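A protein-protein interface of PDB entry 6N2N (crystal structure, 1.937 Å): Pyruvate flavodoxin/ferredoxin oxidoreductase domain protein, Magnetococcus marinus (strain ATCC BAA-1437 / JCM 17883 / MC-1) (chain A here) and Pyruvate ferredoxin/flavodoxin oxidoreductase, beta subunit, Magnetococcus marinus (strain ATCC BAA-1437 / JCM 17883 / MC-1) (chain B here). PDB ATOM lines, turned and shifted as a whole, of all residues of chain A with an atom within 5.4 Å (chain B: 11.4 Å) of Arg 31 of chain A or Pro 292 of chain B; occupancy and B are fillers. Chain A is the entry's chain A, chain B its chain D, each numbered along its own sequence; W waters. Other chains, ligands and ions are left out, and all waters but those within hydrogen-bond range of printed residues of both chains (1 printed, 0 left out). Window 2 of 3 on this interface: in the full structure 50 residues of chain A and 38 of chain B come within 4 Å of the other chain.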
ATOM      1  N   ALA A  26      -5.944  -2.055  -2.402  1.00  0.00           N
ATOM      2  CA  ALA A  26      -7.056  -1.166  -2.081  1.00  0.00           C
ATOM      3  C   ALA A  26      -8.387  -1.805  -2.452  1.00  0.00           C
ATOM      4  O   ALA A  26      -9.332  -1.815  -1.653  1.00  0.00           O
ATOM      5  CB  ALA A  26      -6.880   0.173  -2.802  1.00  0.00           C
ATOM      6  N   ALA A  27      -8.476  -2.356  -3.666  1.00  0.00           N
ATOM      7  CA  ALA A  27      -9.722  -2.974  -4.103  1.00  0.00           C
ATOM      8  C   ALA A  27     -10.052  -4.198  -3.259  1.00  0.00           C
ATOM      9  O   ALA A  27     -11.214  -4.401  -2.884  1.00  0.00           O
ATOM     10  CB  ALA A  27      -9.634  -3.344  -5.582  1.00  0.00           C
ATOM     11  N   ALA A  28      -9.040  -5.013  -2.935  1.00  0.00           N
ATOM     12  CA  ALA A  28      -9.280  -6.200  -2.122  1.00  0.00           C
ATOM     13  C   ALA A  28      -9.796  -5.825  -0.739  1.00  0.00           C
ATOM     14  O   ALA A  28     -10.717  -6.463  -0.217  1.00  0.00           O
ATOM     15  CB  ALA A  28      -8.002  -7.033  -2.015  1.00  0.00           C
ATOM     16  N   CYS A  29      -9.212  -4.796  -0.126  1.00  0.00           N
ATOM     17  CA  CYS A  29      -9.666  -4.381   1.197  1.00  0.00           C
ATOM     18  C   CYS A  29     -11.076  -3.808   1.150  1.00  0.00           C
ATOM     19  O   CYS A  29     -11.864  -4.016   2.081  1.00  0.00           O
ATOM     20  CB  CYS A  29      -8.677  -3.379   1.801  1.00  0.00           C
ATOM     21  SG  CYS A  29      -7.070  -4.157   2.223  1.00  0.00           S
ATOM     22  N   ALA A  30     -11.424  -3.101   0.069  1.00  0.00           N
ATOM     23  CA  ALA A  30     -12.788  -2.599  -0.064  1.00  0.00           C
ATOM     24  C   ALA A  30     -13.776  -3.742  -0.255  1.00  0.00           C
ATOM     25  O   ALA A  30     -14.840  -3.758   0.374  1.00  0.00           O
ATOM     26  CB  ALA A  30     -12.880  -1.611  -1.225  1.00  0.00           C
ATOM     27  N   ARG A  31     -13.437  -4.716  -1.110  1.00  0.00           N
ATOM     28  CA  ARG A  31     -14.279  -5.901  -1.272  1.00  0.00           C
ATOM     29  C   ARG A  31     -14.405  -6.701   0.020  1.00  0.00           C
ATOM     30  O   ARG A  31     -15.353  -7.478   0.166  1.00  0.00           O
ATOM     31  CB  ARG A  31     -13.720  -6.798  -2.371  1.00  0.00           C
ATOM     32  CG  ARG A  31     -13.897  -6.265  -3.775  1.00  0.00           C
ATOM     33  CD  ARG A  31     -13.106  -7.138  -4.728  1.00  0.00           C
ATOM     34  NE  ARG A  31     -13.201  -6.719  -6.121  1.00  0.00           N
ATOM     35  CZ  ARG A  31     -13.767  -7.438  -7.082  1.00  0.00           C
ATOM     36  NH1 ARG A  31     -13.790  -6.976  -8.326  1.00  0.00           N
ATOM     37  NH2 ARG A  31     -14.271  -8.634  -6.807  1.00  0.00           N
ATOM     38  N   ALA A  32     -13.461  -6.549   0.944  1.00  0.00           N
ATOM     39  CA  ALA A  32     -13.533  -7.183   2.252  1.00  0.00           C
ATOM     40  C   ALA A  32     -14.185  -6.282   3.298  1.00  0.00           C
ATOM     41  O   ALA A  32     -14.007  -6.507   4.500  1.00  0.00           O
ATOM     42  CB  ALA A  32     -12.135  -7.617   2.706  1.00  0.00           C
ATOM     43  N   GLY A  33     -14.932  -5.267   2.861  1.00  0.00           N
ATOM     44  CA  GLY A  33     -15.706  -4.426   3.757  1.00  0.00           C
ATOM     45  C   GLY A  33     -14.917  -3.406   4.542  1.00  0.00           C
ATOM     46  O   GLY A  33     -15.383  -2.954   5.590  1.00  0.00           O
ATOM     47  N   THR A 149     -10.468 -12.032  -1.523  1.00  0.00           N
ATOM     48  CA  THR A 149     -10.797 -10.890  -2.379  1.00  0.00           C
ATOM     49  C   THR A 149      -9.606 -10.461  -3.230  1.00  0.00           C
ATOM     50  O   THR A 149      -9.794  -9.901  -4.315  1.00  0.00           O
ATOM     51  CB  THR A 149     -11.318  -9.697  -1.569  1.00  0.00           C
ATOM     52  OG1 THR A 149     -10.292  -9.183  -0.717  1.00  0.00           O
ATOM     53  CG2 THR A 149     -12.526 -10.093  -0.726  1.00  0.00           C
ATOM     54  N   GLU A 152      -9.947 -12.658  -6.118  1.00  0.00           N
ATOM     55  CA  GLU A 152     -11.066 -12.110  -6.887  1.00  0.00           C
ATOM     56  C   GLU A 152     -10.616 -10.944  -7.757  1.00  0.00           C
ATOM     57  O   GLU A 152     -10.932 -10.883  -8.952  1.00  0.00           O
ATOM     58  CB  GLU A 152     -12.191 -11.657  -5.956  1.00  0.00           C
ATOM     59  CG  GLU A 152     -12.993 -12.776  -5.323  1.00  0.00           C
ATOM     60  CD  GLU A 152     -14.104 -12.247  -4.433  1.00  0.00           C
ATOM     61  OE1 GLU A 152     -14.703 -13.048  -3.686  1.00  0.00           O
ATOM     62  OE2 GLU A 152     -14.379 -11.027  -4.487  1.00  0.00           O
ATOM     63  N   VAL A 153      -9.883  -9.997  -7.164  1.00  0.00           N
ATOM     64  CA  VAL A 153      -9.405  -8.835  -7.903  1.00  0.00           C
ATOM     65  C   VAL A 153      -8.457  -9.258  -9.021  1.00  0.00           C
ATOM     66  O   VAL A 153      -8.562  -8.779 -10.155  1.00  0.00           O
ATOM     67  CB  VAL A 153      -8.740  -7.839  -6.935  1.00  0.00           C
ATOM     68  CG1 VAL A 153      -8.011  -6.792  -7.702  1.00  0.00           C
ATOM     69  CG2 VAL A 153      -9.781  -7.187  -6.043  1.00  0.00           C
ATOM     70  N   ASP A 156     -10.473 -10.814 -11.865  1.00  0.00           N
ATOM     71  CA  ASP A 156     -11.132  -9.826 -12.720  1.00  0.00           C
ATOM     72  C   ASP A 156     -10.159  -9.183 -13.699  1.00  0.00           C
ATOM     73  O   ASP A 156     -10.541  -8.855 -14.828  1.00  0.00           O
ATOM     74  CB  ASP A 156     -11.805  -8.736 -11.881  1.00  0.00           C
ATOM     75  CG  ASP A 156     -13.024  -9.234 -11.138  1.00  0.00           C
ATOM     76  OD1 ASP A 156     -13.432 -10.393 -11.360  1.00  0.00           O
ATOM     77  OD2 ASP A 156     -13.578  -8.461 -10.323  1.00  0.00           O
ATOM     78  N   GLN A 195     -15.198  -7.738   6.675  1.00  0.00           N
ATOM     79  CA  GLN A 195     -16.576  -7.443   7.048  1.00  0.00           C
ATOM     80  C   GLN A 195     -17.459  -7.578   5.813  1.00  0.00           C
ATOM     81  O   GLN A 195     -16.977  -7.793   4.695  1.00  0.00           O
ATOM     82  CB  GLN A 195     -16.713  -6.032   7.636  1.00  0.00           C
ATOM     83  CG  GLN A 195     -15.698  -5.698   8.713  1.00  0.00           C
ATOM     84  CD  GLN A 195     -15.754  -4.240   9.140  1.00  0.00           C
ATOM     85  OE1 GLN A 195     -16.390  -3.406   8.488  1.00  0.00           O
ATOM     86  NE2 GLN A 195     -15.064  -3.919  10.227  1.00  0.00           N
ATOM     87  N   PRO A 197     -19.197  -6.503   2.654  1.00  0.00           N
ATOM     88  CA  PRO A 197     -18.851  -5.412   1.734  1.00  0.00           C
ATOM     89  C   PRO A 197     -19.910  -4.316   1.757  1.00  0.00           C
ATOM     90  O   PRO A 197     -21.114  -4.585   1.771  1.00  0.00           O
ATOM     91  CB  PRO A 197     -18.775  -6.105   0.366  1.00  0.00           C
ATOM     92  CG  PRO A 197     -19.501  -7.396   0.536  1.00  0.00           C
ATOM     93  CD  PRO A 197     -19.334  -7.795   1.965  1.00  0.00           C
ATOM     94  N   VAL A 200     -20.187   0.876  -1.705  1.00  0.00           N
ATOM     95  CA  VAL A 200     -19.164   1.887  -1.921  1.00  0.00           C
ATOM     96  C   VAL A 200     -18.653   1.806  -3.353  1.00  0.00           C
ATOM     97  O   VAL A 200     -18.892   0.835  -4.077  1.00  0.00           O
ATOM     98  CB  VAL A 200     -17.983   1.748  -0.927  1.00  0.00           C
ATOM     99  CG1 VAL A 200     -18.460   1.965   0.504  1.00  0.00           C
ATOM    100  CG2 VAL A 200     -17.280   0.385  -1.083  1.00  0.00           C
ATOM    101  N   ILE A 201     -17.951   2.864  -3.761  1.00  0.00           N
ATOM    102  CA  ILE A 201     -17.068   2.821  -4.916  1.00  0.00           C
ATOM    103  C   ILE A 201     -15.702   3.316  -4.462  1.00  0.00           C
ATOM    104  O   ILE A 201     -15.559   3.909  -3.389  1.00  0.00           O
ATOM    105  CB  ILE A 201     -17.580   3.666  -6.107  1.00  0.00           C
ATOM    106  CG1 ILE A 201     -17.623   5.150  -5.736  1.00  0.00           C
ATOM    107  CG2 ILE A 201     -18.952   3.181  -6.567  1.00  0.00           C
ATOM    108  CD1 ILE A 201     -17.925   6.065  -6.918  1.00  0.00           C
ATOM    109  N   ILE A 202     -14.695   3.053  -5.291  1.00  0.00           N
ATOM    110  CA  ILE A 202     -13.351   3.591  -5.118  1.00  0.00           C
ATOM    111  C   ILE A 202     -13.083   4.544  -6.272  1.00  0.00           C
ATOM    112  O   ILE A 202     -13.235   4.170  -7.441  1.00  0.00           O
ATOM    113  CB  ILE A 202     -12.293   2.475  -5.076  1.00  0.00           C
ATOM    114  CG1 ILE A 202     -12.408   1.665  -3.786  1.00  0.00           C
ATOM    115  CG2 ILE A 202     -10.881   3.049  -5.232  1.00  0.00           C
ATOM    116  CD1 ILE A 202     -11.308   0.622  -3.644  1.00  0.00           C
ATOM    117  N   ILE B 286     -22.373   4.667 -15.414  1.00  0.00           N
ATOM    118  CA  ILE B 286     -21.056   5.285 -15.275  1.00  0.00           C
ATOM    119  C   ILE B 286     -20.509   5.044 -13.876  1.00  0.00           C
ATOM    120  O   ILE B 286     -19.336   4.689 -13.698  1.00  0.00           O
ATOM    121  CB  ILE B 286     -21.139   6.789 -15.589  1.00  0.00           C
ATOM    122  CG1 ILE B 286     -21.612   7.009 -17.028  1.00  0.00           C
ATOM    123  CG2 ILE B 286     -19.783   7.456 -15.361  1.00  0.00           C
ATOM    124  CD1 ILE B 286     -22.095   8.414 -17.287  1.00  0.00           C
ATOM    125  N   ILE B 287     -21.355   5.246 -12.863  1.00  0.00           N
ATOM    126  CA  ILE B 287     -20.947   5.075 -11.471  1.00  0.00           C
ATOM    127  C   ILE B 287     -20.480   3.645 -11.219  1.00  0.00           C
ATOM    128  O   ILE B 287     -19.496   3.417 -10.504  1.00  0.00           O
ATOM    129  CB  ILE B 287     -22.110   5.472 -10.541  1.00  0.00           C
ATOM    130  CG1 ILE B 287     -22.460   6.947 -10.732  1.00  0.00           C
ATOM    131  CG2 ILE B 287     -21.780   5.189  -9.077  1.00  0.00           C
ATOM    132  CD1 ILE B 287     -23.733   7.358 -10.026  1.00  0.00           C
ATOM    133  N   ALA B 288     -21.167   2.664 -11.815  1.00  0.00           N
ATOM    134  CA  ALA B 288     -20.863   1.260 -11.556  1.00  0.00           C
ATOM    135  C   ALA B 288     -19.444   0.896 -11.971  1.00  0.00           C
ATOM    136  O   ALA B 288     -18.856  -0.032 -11.408  1.00  0.00           O
ATOM    137  CB  ALA B 288     -21.869   0.359 -12.274  1.00  0.00           C
ATOM    138  N   LEU B 289     -18.866   1.627 -12.927  1.00  0.00           N
ATOM    139  CA  LEU B 289     -17.501   1.345 -13.360  1.00  0.00           C
ATOM    140  C   LEU B 289     -16.483   1.561 -12.248  1.00  0.00           C
ATOM    141  O   LEU B 289     -15.361   1.047 -12.342  1.00  0.00           O
ATOM    142  CB  LEU B 289     -17.149   2.219 -14.565  1.00  0.00           C
ATOM    143  CG  LEU B 289     -18.026   2.006 -15.802  1.00  0.00           C
ATOM    144  CD1 LEU B 289     -17.743   3.062 -16.857  1.00  0.00           C
ATOM    145  CD2 LEU B 289     -17.820   0.606 -16.377  1.00  0.00           C
ATOM    146  N   ALA B 290     -16.837   2.305 -11.204  1.00  0.00           N
ATOM    147  CA  ALA B 290     -15.915   2.584 -10.111  1.00  0.00           C
ATOM    148  C   ALA B 290     -16.046   1.613  -8.939  1.00  0.00           C
ATOM    149  O   ALA B 290     -15.372   1.805  -7.921  1.00  0.00           O
ATOM    150  CB  ALA B 290     -16.109   4.021  -9.612  1.00  0.00           C
ATOM    151  N   LYS B 291     -16.891   0.588  -9.043  1.00  0.00           N
ATOM    152  CA  LYS B 291     -17.029  -0.363  -7.948  1.00  0.00           C
ATOM    153  C   LYS B 291     -15.738  -1.165  -7.791  1.00  0.00           C
ATOM    154  O   LYS B 291     -15.108  -1.526  -8.789  1.00  0.00           O
ATOM    155  CB  LYS B 291     -18.209  -1.304  -8.196  1.00  0.00           C
ATOM    156  CG  LYS B 291     -19.567  -0.615  -8.134  1.00  0.00           C
ATOM    157  CD  LYS B 291     -20.713  -1.576  -8.405  1.00  0.00           C
ATOM    158  CE  LYS B 291     -22.050  -0.855  -8.309  1.00  0.00           C
ATOM    159  NZ  LYS B 291     -23.219  -1.773  -8.467  1.00  0.00           N
ATOM    160  N   PRO B 292     -15.307  -1.443  -6.550  1.00  0.00           N
ATOM    161  CA  PRO B 292     -14.046  -2.152  -6.285  1.00  0.00           C
ATOM    162  C   PRO B 292     -14.011  -3.548  -6.899  1.00  0.00           C
ATOM    163  O   PRO B 292     -15.040  -4.199  -7.065  1.00  0.00           O
ATOM    164  CB  PRO B 292     -13.994  -2.227  -4.753  1.00  0.00           C
ATOM    165  CG  PRO B 292     -15.395  -1.936  -4.287  1.00  0.00           C
ATOM    166  CD  PRO B 292     -15.984  -1.030  -5.309  1.00  0.00           C
ATOM    167  OXT PRO B 292     -12.948  -4.052  -7.263  1.00  0.00           O
HETATM  168  O   HOH W   1     -12.275   1.635  -8.697  1.00  0.00           O
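Among the printed residues, merely in contact across the chains: Ile 201 of chain A with Ala 290 of chain B (3.4 Å), Val 200 of chain A with Pro 292 of chain B (3.7 Å), Ala 30 of chain A with Pro 292 of chain B (3.8 Å), Ala 27 of chain A with Pro 292 of chain B (3.8 Å) and Ile 201 of chain A with Ile 287 of chain B (3.98 Å).
Water W1 bridges the backbone carbonyl oxygen of Ile 202 of chain A (3.0 Å) and the backbone carbonyl oxygen of Ala 290 of chain B (3.2 Å).
Hydrophobic or aromatic side chains of chain A within 4 Å of the printed part of chain B: Ala 27, Ala 30 and Ile 201. Of the 7 printed residues of chain B, 3 touch a printed residue of chain A. Printed residues of chain B that touch a printed residue of chain A: Ile 287, Ala 290 and Pro 292. Among the printed residues, no Asp or Glu carboxylate lies within 4 Å of a Lys or Arg side-chain nitrogen of the other chain.
The guanidinium group (NH2) of Arg 31 of chain A is in salt-bridge range of the side-chain carboxylate (OE2) of Glu 152 of chain A (3.3 Å). The guanidinium group (NH1) of Arg 31 of chain A is in salt-bridge range of the side-chain carboxylate (OD2) of Asp 156 of chain A (2.5 Å).
The backbone NH (N) of Ile 202 of chain A is in hydrogen-bond range of the backbone carbonyl oxygen (O) of Ala 290 of chain B. The chain-end carboxylate of Pro 292 of chain B lies within salt-bridge range of the guanidinium group of Arg 31 of chain A, at 2.9 Å.
Ala 27 of chain A touches just one residue of chain B: Pro 292 (3.8 Å). No residue of chain B comes within 4 Å of Ala 28 of chain A. No residue of chain B comes within 4 Å of Cys 29 of chain A. Ala 30 of chain A touches just one residue of chain B: Pro 292 (3.8 Å). Of chain B, only Pro 292 comes within 4 Å of Arg 31 of chain A. No residue of chain B comes within 4 Å of Ala 32 of chain A. No residue of chain B comes within 4 Å of Thr 149 of chain A. No residue of chain B comes within 4 Å of Glu 152 of chain A. No residue of chain B comes within 4 Å of Val 153 of chain A. Gln 195 of chain A touches none of the printed residues of chain B. No residue of chain B comes within 4 Å of Pro 197 of chain A. Printed residues of chain B within 4 Å of Ile 201 of chain A: Ile 287 (3.98 Å) and Ala 290 (3.4 Å). Of chain B, only Ala 290 (3.0 Å) comes within 4 Å of Ile 202 of chain A. Printed residues of chain A within 4 Å of Ile 287 of chain B: Ile 201. Printed residues of chain A within 4 Å of Ala 290 of chain B: Ile 201 (3.4 Å) and Ile 202 (3.0 Å). Of the printed residues of chain A, Pro 292 of chain B touches Ala 27, Ala 30, Arg 31 and Val 200. The nearest printed residue of chain A that does not touch Pro 292 of chain B is Ile 201 of chain A (4.02 Å).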
